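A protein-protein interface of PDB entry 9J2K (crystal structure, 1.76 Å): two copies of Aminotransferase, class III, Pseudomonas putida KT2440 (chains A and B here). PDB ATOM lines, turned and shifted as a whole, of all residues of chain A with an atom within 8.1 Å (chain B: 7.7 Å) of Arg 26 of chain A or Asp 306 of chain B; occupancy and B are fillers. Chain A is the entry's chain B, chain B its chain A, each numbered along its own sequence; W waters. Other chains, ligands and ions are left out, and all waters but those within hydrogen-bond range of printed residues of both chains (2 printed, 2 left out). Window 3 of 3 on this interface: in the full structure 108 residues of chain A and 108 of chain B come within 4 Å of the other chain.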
ATOM      1  N   HIS A   4       8.964  15.560  -8.311  1.00  0.00           N
ATOM      2  CA  HIS A   4       8.190  14.330  -8.264  1.00  0.00           C
ATOM      3  C   HIS A   4       8.041  13.738  -9.664  1.00  0.00           C
ATOM      4  O   HIS A   4       8.116  14.444 -10.673  1.00  0.00           O
ATOM      5  CB  HIS A   4       6.805  14.593  -7.667  1.00  0.00           C
ATOM      6  CG  HIS A   4       6.828  15.028  -6.232  1.00  0.00           C
ATOM      7  ND1 HIS A   4       5.734  15.593  -5.611  1.00  0.00           N
ATOM      8  CD2 HIS A   4       7.805  14.970  -5.296  1.00  0.00           C
ATOM      9  CE1 HIS A   4       6.037  15.870  -4.355  1.00  0.00           C
ATOM     10  NE2 HIS A   4       7.288  15.503  -4.138  1.00  0.00           N
ATOM     11  N   ASP A  11      -1.224  11.650  -9.482  1.00  0.00           N
ATOM     12  CA  ASP A  11      -1.910  11.144  -8.299  1.00  0.00           C
ATOM     13  C   ASP A  11      -2.317  12.283  -7.367  1.00  0.00           C
ATOM     14  O   ASP A  11      -3.489  12.399  -6.980  1.00  0.00           O
ATOM     15  CB  ASP A  11      -0.990  10.145  -7.592  1.00  0.00           C
ATOM     16  CG  ASP A  11      -1.583   9.592  -6.301  1.00  0.00           C
ATOM     17  OD1 ASP A  11      -1.688  10.349  -5.318  1.00  0.00           O
ATOM     18  OD2 ASP A  11      -1.919   8.385  -6.265  1.00  0.00           O
ATOM     19  N   LEU A  12      -1.362  13.147  -7.010  1.00  0.00           N
ATOM     20  CA  LEU A  12      -1.642  14.224  -6.063  1.00  0.00           C
ATOM     21  C   LEU A  12      -2.694  15.184  -6.596  1.00  0.00           C
ATOM     22  O   LEU A  12      -3.465  15.764  -5.814  1.00  0.00           O
ATOM     23  CB  LEU A  12      -0.354  14.991  -5.736  1.00  0.00           C
ATOM     24  CG  LEU A  12       0.653  14.258  -4.844  1.00  0.00           C
ATOM     25  CD1 LEU A  12       1.996  15.008  -4.822  1.00  0.00           C
ATOM     26  CD2 LEU A  12       0.082  14.105  -3.444  1.00  0.00           C
ATOM     27  N   ALA A  13      -2.753  15.362  -7.917  1.00  0.00           N
ATOM     28  CA  ALA A  13      -3.705  16.312  -8.476  1.00  0.00           C
ATOM     29  C   ALA A  13      -5.120  15.754  -8.494  1.00  0.00           C
ATOM     30  O   ALA A  13      -6.074  16.485  -8.209  1.00  0.00           O
ATOM     31  CB  ALA A  13      -3.299  16.718  -9.893  1.00  0.00           C
ATOM     32  N   ILE A  16      -8.505  10.211  -5.799  1.00  0.00           N
ATOM     33  CA  ILE A  16      -9.033   9.982  -4.454  1.00  0.00           C
ATOM     34  C   ILE A  16      -8.728   8.541  -4.066  1.00  0.00           C
ATOM     35  O   ILE A  16      -9.210   7.604  -4.712  1.00  0.00           O
ATOM     36  CB  ILE A  16     -10.545  10.241  -4.388  1.00  0.00           C
ATOM     37  CG1 ILE A  16     -10.882  11.668  -4.822  1.00  0.00           C
ATOM     38  CG2 ILE A  16     -11.071   9.958  -2.976  1.00  0.00           C
ATOM     39  CD1 ILE A  16     -12.369  11.887  -5.045  1.00  0.00           C
ATOM     40  N   THR A  20      -7.574   5.305   2.724  1.00  0.00           N
ATOM     41  CA  THR A  20      -6.361   6.089   2.864  1.00  0.00           C
ATOM     42  C   THR A  20      -6.704   7.342   3.652  1.00  0.00           C
ATOM     43  O   THR A  20      -7.813   7.869   3.543  1.00  0.00           O
ATOM     44  CB  THR A  20      -5.789   6.481   1.487  1.00  0.00           C
ATOM     45  OG1 THR A  20      -5.394   5.298   0.770  1.00  0.00           O
ATOM     46  CG2 THR A  20      -4.603   7.450   1.595  1.00  0.00           C
ATOM     47  N   ASN A  21      -5.750   7.827   4.438  1.00  0.00           N
ATOM     48  CA  ASN A  21      -5.921   9.125   5.084  1.00  0.00           C
ATOM     49  C   ASN A  21      -5.695  10.186   4.012  1.00  0.00           C
ATOM     50  O   ASN A  21      -4.558  10.484   3.643  1.00  0.00           O
ATOM     51  CB  ASN A  21      -4.963   9.277   6.263  1.00  0.00           C
ATOM     52  CG  ASN A  21      -5.163  10.584   7.015  1.00  0.00           C
ATOM     53  OD1 ASN A  21      -5.478  11.619   6.424  1.00  0.00           O
ATOM     54  ND2 ASN A  21      -4.987  10.538   8.336  1.00  0.00           N
ATOM     55  N   LEU A  22      -6.789  10.756   3.509  1.00  0.00           N
ATOM     56  CA  LEU A  22      -6.705  11.695   2.393  1.00  0.00           C
ATOM     57  C   LEU A  22      -5.998  12.996   2.773  1.00  0.00           C
ATOM     58  O   LEU A  22      -5.404  13.650   1.903  1.00  0.00           O
ATOM     59  CB  LEU A  22      -8.109  11.997   1.859  1.00  0.00           C
ATOM     60  CG  LEU A  22      -8.934  10.780   1.438  1.00  0.00           C
ATOM     61  CD1 LEU A  22     -10.313  11.224   0.972  1.00  0.00           C
ATOM     62  CD2 LEU A  22      -8.204   9.967   0.363  1.00  0.00           C
ATOM     63  N   ALA A  23      -6.076  13.411   4.043  1.00  0.00           N
ATOM     64  CA  ALA A  23      -5.350  14.606   4.474  1.00  0.00           C
ATOM     65  C   ALA A  23      -3.848  14.353   4.499  1.00  0.00           C
ATOM     66  O   ALA A  23      -3.064  15.134   3.943  1.00  0.00           O
ATOM     67  CB  ALA A  23      -5.834  15.059   5.855  1.00  0.00           C
ATOM     68  N   GLN A  24      -3.425  13.262   5.145  1.00  0.00           N
ATOM     69  CA  GLN A  24      -2.011  12.914   5.122  1.00  0.00           C
ATOM     70  C   GLN A  24      -1.515  12.690   3.701  1.00  0.00           C
ATOM     71  O   GLN A  24      -0.348  12.966   3.402  1.00  0.00           O
ATOM     72  CB  GLN A  24      -1.758  11.668   5.974  1.00  0.00           C
ATOM     73  CG  GLN A  24      -1.701  11.957   7.468  1.00  0.00           C
ATOM     74  CD  GLN A  24      -0.492  12.801   7.839  1.00  0.00           C
ATOM     75  OE1 GLN A  24       0.644  12.319   7.823  1.00  0.00           O
ATOM     76  NE2 GLN A  24      -0.729  14.068   8.165  1.00  0.00           N
ATOM     77  N   HIS A  25      -2.385  12.214   2.805  1.00  0.00           N
ATOM     78  CA  HIS A  25      -1.943  11.930   1.446  1.00  0.00           C
ATOM     79  C   HIS A  25      -1.449  13.191   0.749  1.00  0.00           C
ATOM     80  O   HIS A  25      -0.482  13.139  -0.016  1.00  0.00           O
ATOM     81  CB  HIS A  25      -3.067  11.281   0.637  1.00  0.00           C
ATOM     82  CG  HIS A  25      -2.589  10.646  -0.628  1.00  0.00           C
ATOM     83  ND1 HIS A  25      -1.950   9.423  -0.649  1.00  0.00           N
ATOM     84  CD2 HIS A  25      -2.627  11.075  -1.913  1.00  0.00           C
ATOM     85  CE1 HIS A  25      -1.627   9.119  -1.894  1.00  0.00           C
ATOM     86  NE2 HIS A  25      -2.019  10.108  -2.679  1.00  0.00           N
ATOM     87  N   ARG A  26      -2.081  14.343   1.025  1.00  0.00           N
ATOM     88  CA  ARG A  26      -1.606  15.602   0.451  1.00  0.00           C
ATOM     89  C   ARG A  26      -0.178  15.915   0.876  1.00  0.00           C
ATOM     90  O   ARG A  26       0.575  16.527   0.105  1.00  0.00           O
ATOM     91  CB  ARG A  26      -2.516  16.763   0.861  1.00  0.00           C
ATOM     92  CG  ARG A  26      -3.890  16.723   0.248  1.00  0.00           C
ATOM     93  CD  ARG A  26      -4.692  17.959   0.619  1.00  0.00           C
ATOM     94  NE  ARG A  26      -5.900  18.054  -0.186  1.00  0.00           N
ATOM     95  CZ  ARG A  26      -6.853  18.965  -0.030  1.00  0.00           C
ATOM     96  NH1 ARG A  26      -6.799  19.870   0.935  1.00  0.00           N
ATOM     97  NH2 ARG A  26      -7.891  18.962  -0.859  1.00  0.00           N
ATOM     98  N   GLU A  27       0.208  15.509   2.088  1.00  0.00           N
ATOM     99  CA  GLU A  27       1.532  15.781   2.641  1.00  0.00           C
ATOM    100  C   GLU A  27       2.579  14.758   2.208  1.00  0.00           C
ATOM    101  O   GLU A  27       3.642  15.135   1.702  1.00  0.00           O
ATOM    102  CB  GLU A  27       1.462  15.826   4.168  1.00  0.00           C
ATOM    103  CG  GLU A  27       0.309  16.650   4.709  1.00  0.00           C
ATOM    104  CD  GLU A  27       0.445  18.136   4.415  1.00  0.00           C
ATOM    105  OE1 GLU A  27       1.522  18.575   3.954  1.00  0.00           O
ATOM    106  OE2 GLU A  27      -0.537  18.869   4.654  1.00  0.00           O
ATOM    107  N   VAL A  28       2.302  13.469   2.412  1.00  0.00           N
ATOM    108  CA  VAL A  28       3.298  12.433   2.151  1.00  0.00           C
ATOM    109  C   VAL A  28       3.236  11.886   0.729  1.00  0.00           C
ATOM    110  O   VAL A  28       4.210  11.275   0.264  1.00  0.00           O
ATOM    111  CB  VAL A  28       3.147  11.286   3.166  1.00  0.00           C
ATOM    112  CG1 VAL A  28       3.224  11.827   4.594  1.00  0.00           C
ATOM    113  CG2 VAL A  28       1.837  10.530   2.948  1.00  0.00           C
ATOM    114  N   GLY A  29       2.126  12.080   0.026  1.00  0.00           N
ATOM    115  CA  GLY A  29       1.998  11.592  -1.325  1.00  0.00           C
ATOM    116  C   GLY A  29       1.922  10.079  -1.425  1.00  0.00           C
ATOM    117  O   GLY A  29       1.928   9.351  -0.420  1.00  0.00           O
ATOM    118  N   PRO A  30       1.846   9.580  -2.655  1.00  0.00           N
ATOM    119  CA  PRO A  30       1.675   8.143  -2.872  1.00  0.00           C
ATOM    120  C   PRO A  30       3.005   7.403  -2.919  1.00  0.00           C
ATOM    121  O   PRO A  30       4.073   7.984  -3.126  1.00  0.00           O
ATOM    122  CB  PRO A  30       0.991   8.088  -4.242  1.00  0.00           C
ATOM    123  CG  PRO A  30       1.639   9.229  -4.969  1.00  0.00           C
ATOM    124  CD  PRO A  30       1.774  10.330  -3.923  1.00  0.00           C
ATOM    125  N   HIS B  87      -2.161   4.729   0.675  1.00  0.00           N
ATOM    126  CA  HIS B  87      -1.336   5.623  -0.140  1.00  0.00           C
ATOM    127  C   HIS B  87      -0.691   4.914  -1.327  1.00  0.00           C
ATOM    128  O   HIS B  87      -0.042   5.592  -2.131  1.00  0.00           O
ATOM    129  CB  HIS B  87      -0.218   6.336   0.650  1.00  0.00           C
ATOM    130  CG  HIS B  87      -0.695   7.047   1.883  1.00  0.00           C
ATOM    131  ND1 HIS B  87      -1.370   8.250   1.836  1.00  0.00           N
ATOM    132  CD2 HIS B  87      -0.580   6.731   3.196  1.00  0.00           C
ATOM    133  CE1 HIS B  87      -1.655   8.643   3.066  1.00  0.00           C
ATOM    134  NE2 HIS B  87      -1.183   7.739   3.911  1.00  0.00           N
ATOM    135  N   HIS B 110     -11.466  15.465  -9.334  1.00  0.00           N
ATOM    136  CA  HIS B 110     -10.983  14.439  -8.418  1.00  0.00           C
ATOM    137  C   HIS B 110     -11.759  13.161  -8.668  1.00  0.00           C
ATOM    138  O   HIS B 110     -12.987  13.196  -8.793  1.00  0.00           O
ATOM    139  CB  HIS B 110     -11.119  14.913  -6.967  1.00  0.00           C
ATOM    140  CG  HIS B 110     -10.365  16.179  -6.713  1.00  0.00           C
ATOM    141  ND1 HIS B 110      -9.023  16.193  -6.394  1.00  0.00           N
ATOM    142  CD2 HIS B 110     -10.744  17.477  -6.806  1.00  0.00           C
ATOM    143  CE1 HIS B 110      -8.615  17.444  -6.272  1.00  0.00           C
ATOM    144  NE2 HIS B 110      -9.637  18.242  -6.522  1.00  0.00           N
ATOM    145  N   VAL B 131     -20.279  13.613   3.204  1.00  0.00           N
ATOM    146  CA  VAL B 131     -19.986  15.037   3.111  1.00  0.00           C
ATOM    147  C   VAL B 131     -21.021  15.845   3.881  1.00  0.00           C
ATOM    148  O   VAL B 131     -20.679  16.807   4.578  1.00  0.00           O
ATOM    149  CB  VAL B 131     -19.902  15.465   1.638  1.00  0.00           C
ATOM    150  CG1 VAL B 131     -20.014  16.990   1.512  1.00  0.00           C
ATOM    151  CG2 VAL B 131     -18.597  14.980   1.040  1.00  0.00           C
ATOM    152  N   ALA B 134     -20.306  15.660   7.463  1.00  0.00           N
ATOM    153  CA  ALA B 134     -19.148  16.505   7.754  1.00  0.00           C
ATOM    154  C   ALA B 134     -19.533  17.976   7.799  1.00  0.00           C
ATOM    155  O   ALA B 134     -18.965  18.756   8.576  1.00  0.00           O
ATOM    156  CB  ALA B 134     -18.059  16.296   6.704  1.00  0.00           C
ATOM    157  N   VAL B 300     -15.653  14.222  -8.929  1.00  0.00           N
ATOM    158  CA  VAL B 300     -16.284  15.165  -8.013  1.00  0.00           C
ATOM    159  C   VAL B 300     -15.531  16.491  -8.032  1.00  0.00           C
ATOM    160  O   VAL B 300     -14.415  16.598  -8.546  1.00  0.00           O
ATOM    161  CB  VAL B 300     -16.369  14.621  -6.570  1.00  0.00           C
ATOM    162  CG1 VAL B 300     -17.011  13.240  -6.554  1.00  0.00           C
ATOM    163  CG2 VAL B 300     -14.980  14.582  -5.919  1.00  0.00           C
ATOM    164  N   SER B 301     -16.155  17.502  -7.428  1.00  0.00           N
ATOM    165  CA  SER B 301     -15.623  18.856  -7.446  1.00  0.00           C
ATOM    166  C   SER B 301     -14.496  19.039  -6.434  1.00  0.00           C
ATOM    167  O   SER B 301     -14.321  18.249  -5.496  1.00  0.00           O
ATOM    168  CB  SER B 301     -16.734  19.870  -7.149  1.00  0.00           C
ATOM    169  OG  SER B 301     -17.166  19.758  -5.798  1.00  0.00           O
ATOM    170  N   ASP B 302     -13.727  20.119  -6.637  1.00  0.00           N
ATOM    171  CA  ASP B 302     -12.746  20.538  -5.640  1.00  0.00           C
ATOM    172  C   ASP B 302     -13.385  20.675  -4.266  1.00  0.00           C
ATOM    173  O   ASP B 302     -12.809  20.247  -3.258  1.00  0.00           O
ATOM    174  CB  ASP B 302     -12.115  21.879  -6.029  1.00  0.00           C
ATOM    175  CG  ASP B 302     -11.202  21.780  -7.227  1.00  0.00           C
ATOM    176  OD1 ASP B 302     -10.618  20.701  -7.462  1.00  0.00           O
ATOM    177  OD2 ASP B 302     -11.057  22.810  -7.928  1.00  0.00           O
ATOM    178  N   ALA B 303     -14.571  21.293  -4.205  1.00  0.00           N
ATOM    179  CA  ALA B 303     -15.208  21.531  -2.908  1.00  0.00           C
ATOM    180  C   ALA B 303     -15.563  20.223  -2.217  1.00  0.00           C
ATOM    181  O   ALA B 303     -15.401  20.089  -0.996  1.00  0.00           O
ATOM    182  CB  ALA B 303     -16.462  22.386  -3.077  1.00  0.00           C
ATOM    183  N   MET B 304     -16.065  19.251  -2.975  1.00  0.00           N
ATOM    184  CA  MET B 304     -16.399  17.970  -2.373  1.00  0.00           C
ATOM    185  C   MET B 304     -15.146  17.249  -1.900  1.00  0.00           C
ATOM    186  O   MET B 304     -15.111  16.706  -0.788  1.00  0.00           O
ATOM    187  CB  MET B 304     -17.161  17.099  -3.362  1.00  0.00           C
ATOM    188  CG  MET B 304     -17.276  15.692  -2.870  1.00  0.00           C
ATOM    189  SD  MET B 304     -18.762  14.972  -3.534  1.00  0.00           S
ATOM    190  CE  MET B 304     -19.951  16.098  -2.790  1.00  0.00           C
ATOM    191  N   ASN B 305     -14.106  17.226  -2.738  1.00  0.00           N
ATOM    192  CA  ASN B 305     -12.841  16.636  -2.326  1.00  0.00           C
ATOM    193  C   ASN B 305     -12.313  17.288  -1.049  1.00  0.00           C
ATOM    194  O   ASN B 305     -11.823  16.596  -0.150  1.00  0.00           O
ATOM    195  CB  ASN B 305     -11.817  16.749  -3.456  1.00  0.00           C
ATOM    196  CG  ASN B 305     -10.515  16.048  -3.122  1.00  0.00           C
ATOM    197  OD1 ASN B 305      -9.451  16.663  -3.062  1.00  0.00           O
ATOM    198  ND2 ASN B 305     -10.603  14.761  -2.875  1.00  0.00           N
ATOM    199  N   ASP B 306     -12.429  18.618  -0.938  1.00  0.00           N
ATOM    200  CA  ASP B 306     -11.963  19.287   0.279  1.00  0.00           C
ATOM    201  C   ASP B 306     -12.681  18.761   1.517  1.00  0.00           C
ATOM    202  O   ASP B 306     -12.073  18.628   2.587  1.00  0.00           O
ATOM    203  CB  ASP B 306     -12.158  20.802   0.175  1.00  0.00           C
ATOM    204  CG  ASP B 306     -11.148  21.463  -0.751  1.00  0.00           C
ATOM    205  OD1 ASP B 306     -10.088  20.863  -1.033  1.00  0.00           O
ATOM    206  OD2 ASP B 306     -11.417  22.605  -1.182  1.00  0.00           O
ATOM    207  N   VAL B 307     -13.976  18.461   1.401  1.00  0.00           N
ATOM    208  CA  VAL B 307     -14.684  17.915   2.555  1.00  0.00           C
ATOM    209  C   VAL B 307     -14.222  16.490   2.839  1.00  0.00           C
ATOM    210  O   VAL B 307     -14.066  16.097   4.002  1.00  0.00           O
ATOM    211  CB  VAL B 307     -16.205  17.985   2.355  1.00  0.00           C
ATOM    212  CG1 VAL B 307     -16.905  17.409   3.582  1.00  0.00           C
ATOM    213  CG2 VAL B 307     -16.639  19.422   2.135  1.00  0.00           C
ATOM    214  N   LEU B 308     -13.986  15.695   1.789  1.00  0.00           N
ATOM    215  CA  LEU B 308     -13.437  14.358   1.997  1.00  0.00           C
ATOM    216  C   LEU B 308     -12.100  14.427   2.724  1.00  0.00           C
ATOM    217  O   LEU B 308     -11.817  13.607   3.604  1.00  0.00           O
ATOM    218  CB  LEU B 308     -13.270  13.628   0.658  1.00  0.00           C
ATOM    219  CG  LEU B 308     -14.524  13.397  -0.180  1.00  0.00           C
ATOM    220  CD1 LEU B 308     -14.137  12.685  -1.488  1.00  0.00           C
ATOM    221  CD2 LEU B 308     -15.596  12.620   0.581  1.00  0.00           C
ATOM    222  N   VAL B 309     -11.267  15.406   2.373  1.00  0.00           N
ATOM    223  CA  VAL B 309      -9.980  15.550   3.039  1.00  0.00           C
ATOM    224  C   VAL B 309     -10.164  15.972   4.494  1.00  0.00           C
ATOM    225  O   VAL B 309      -9.477  15.459   5.390  1.00  0.00           O
ATOM    226  CB  VAL B 309      -9.092  16.535   2.262  1.00  0.00           C
ATOM    227  CG1 VAL B 309      -7.892  16.961   3.113  1.00  0.00           C
ATOM    228  CG2 VAL B 309      -8.646  15.894   0.949  1.00  0.00           C
ATOM    229  N   SER B 310     -11.090  16.901   4.765  1.00  0.00           N
ATOM    230  CA  SER B 310     -11.276  17.323   6.152  1.00  0.00           C
ATOM    231  C   SER B 310     -11.809  16.176   7.009  1.00  0.00           C
ATOM    232  O   SER B 310     -11.498  16.100   8.204  1.00  0.00           O
ATOM    233  CB  SER B 310     -12.191  18.561   6.233  1.00  0.00           C
ATOM    234  OG  SER B 310     -13.549  18.290   5.920  1.00  0.00           O
ATOM    235  N   GLN B 311     -12.570  15.254   6.409  1.00  0.00           N
ATOM    236  CA  GLN B 311     -13.035  14.074   7.140  1.00  0.00           C
ATOM    237  C   GLN B 311     -11.885  13.155   7.525  1.00  0.00           C
ATOM    238  O   GLN B 311     -11.857  12.633   8.647  1.00  0.00           O
ATOM    239  CB  GLN B 311     -14.051  13.291   6.314  1.00  0.00           C
ATOM    240  CG  GLN B 311     -15.429  13.910   6.287  1.00  0.00           C
ATOM    241  CD  GLN B 311     -16.162  13.722   7.604  1.00  0.00           C
ATOM    242  OE1 GLN B 311     -15.895  14.421   8.587  1.00  0.00           O
ATOM    243  NE2 GLN B 311     -17.089  12.771   7.630  1.00  0.00           N
ATOM    244  N   SER B 312     -10.959  12.898   6.590  1.00  0.00           N
ATOM    245  CA  SER B 312      -9.806  12.063   6.914  1.00  0.00           C
ATOM    246  C   SER B 312      -8.989  12.679   8.040  1.00  0.00           C
ATOM    247  O   SER B 312      -8.408  11.962   8.864  1.00  0.00           O
ATOM    248  CB  SER B 312      -8.935  11.846   5.674  1.00  0.00           C
ATOM    249  OG  SER B 312      -9.344  10.687   4.963  1.00  0.00           O
HETATM  250  O   HOH W   1      -6.553  16.419  -2.539  1.00  0.00           O
HETATM  251  O   HOH W   2      -3.589   5.850   5.055  1.00  0.00           O
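The backbone NH (N) of His 87 of chain B sits at hydrogen-bond distance from the side-chain hydroxyl (OG1) of Thr 20 of chain A (3.3 Å).
N of Leu 22 of chain A is in hydrogen-bond range of OG of Ser 312 of chain B (2.9 Å).
NH2 of Arg 26 of chain A lies within salt-bridge range of OD1 of Asp 306 of chain B (2.9 Å).
A ring nitrogen (ND1) of His 110 of chain B lies close to the backbone carbonyl oxygen (O) of Ala 13 of chain A (3.5 Å).
A ring nitrogen (ND1) of His 87 of chain B is in hydrogen-bond range of a ring nitrogen (ND1) of His 25 of chain A, 2.8 Å away.
The side-chain amide oxygen (OD1) of Asn 21 of chain A sits at hydrogen-bond distance from the backbone NH (N) of Gln 24 of chain A (2.9 Å).
NE2 of His 110 of chain B sits at hydrogen-bond distance from OD1 of Asp 302 of chain B (2.8 Å).
The backbone carbonyl oxygen (O) of His 110 of chain B is in hydrogen-bond range of the backbone NH (N) of Val 300 of chain B, 2.9 Å away.
A ring nitrogen (ND1) of His 110 of chain B sits at hydrogen-bond distance from the side-chain amide oxygen (OD1) of Asn 305 of chain B, at 3.4 Å.
A ring nitrogen (NE2) of His 25 of chain A lies within hydrogen-bond range of the side-chain carboxylate (OD1) of Asp 11 of chain A, 2.7 Å away.
OD1 of Asn 21 of chain A lies within hydrogen-bond range of N of Ala 23 of chain A (3.0 Å).
Among the printed residues, merely in contact across the chains: Pro 30 of chain A with His 87 of chain B (3.2 Å), Asn 21 of chain A with His 87 of chain B (3.5 Å), Thr 20 of chain A with Ser 312 of chain B (3.5 Å), Asn 21 of chain A with Ser 312 of chain B (3.5 Å), Arg 26 of chain A with Asn 305 of chain B (3.5 Å), Arg 26 of chain A with Val 309 of chain B (3.6 Å), Ala 23 of chain A with Ser 312 of chain B (3.6 Å), Ile 16 of chain A with Asn 305 of chain B (3.7 Å), Ala 23 of chain A with Val 309 of chain B (3.7 Å), Ile 16 of chain A with His 110 of chain B (3.8 Å), Leu 22 of chain A with Leu 308 of chain B (3.8 Å), Gly 29 of chain A with His 87 of chain B (3.9 Å), Ile 16 of chain A with Val 300 of chain B (3.9 Å) and Val 28 of chain A with His 87 of chain B (3.97 Å).
Arg 26 of chain A touches just these residues of chain B: Asn 305, Asp 306 and Val 309.
Asp 306 of chain B touches just one residue of chain A: Arg 26 (2.9 Å).
Printed residues of chain A within 4 Å of His 110 of chain B: Ala 13 and Ile 16.
Of the printed residues of chain B, His 25 of chain A touches His 87 (2.8 Å).
Of the printed residues of chain B, Leu 22 of chain A touches Leu 308 and Ser 312.
Glu 27 of chain A touches none of the printed residues of chain B.
Ala 134 of chain B touches none of the printed residues of chain A.
The nearest printed residue of chain B that does not touch Val 28 of chain A is Val 309 of chain B (10.8 Å).
Of the 17 printed residues of chain B, 8 touch a printed residue of chain A.
Hydrophobic or aromatic side chains of chain B that line the printed part of chain A: His 87, His 110, Val 300, Leu 308 and Val 309.
Hydrophobic or aromatic side chains of chain A that line the printed part of chain B: Ile 16, Leu 22, Ala 23, His 25, Val 28 and Pro 30.
Among the printed residues, 19 pairs touch across the chains.
No position is printed for both chains.
Of the 19 pairs that touch across the chains among the printed residues, none has its exchanged pair printed and touching as well.
Water W1 lies within hydrogen-bond range of NE of Arg 26 of chain A (2.9 Å) and OD1 of Asn 305 of chain B (3.0 Å).
Water W2 bridges N of Asn 21 of chain A and NE2 of His 87 of chain B.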
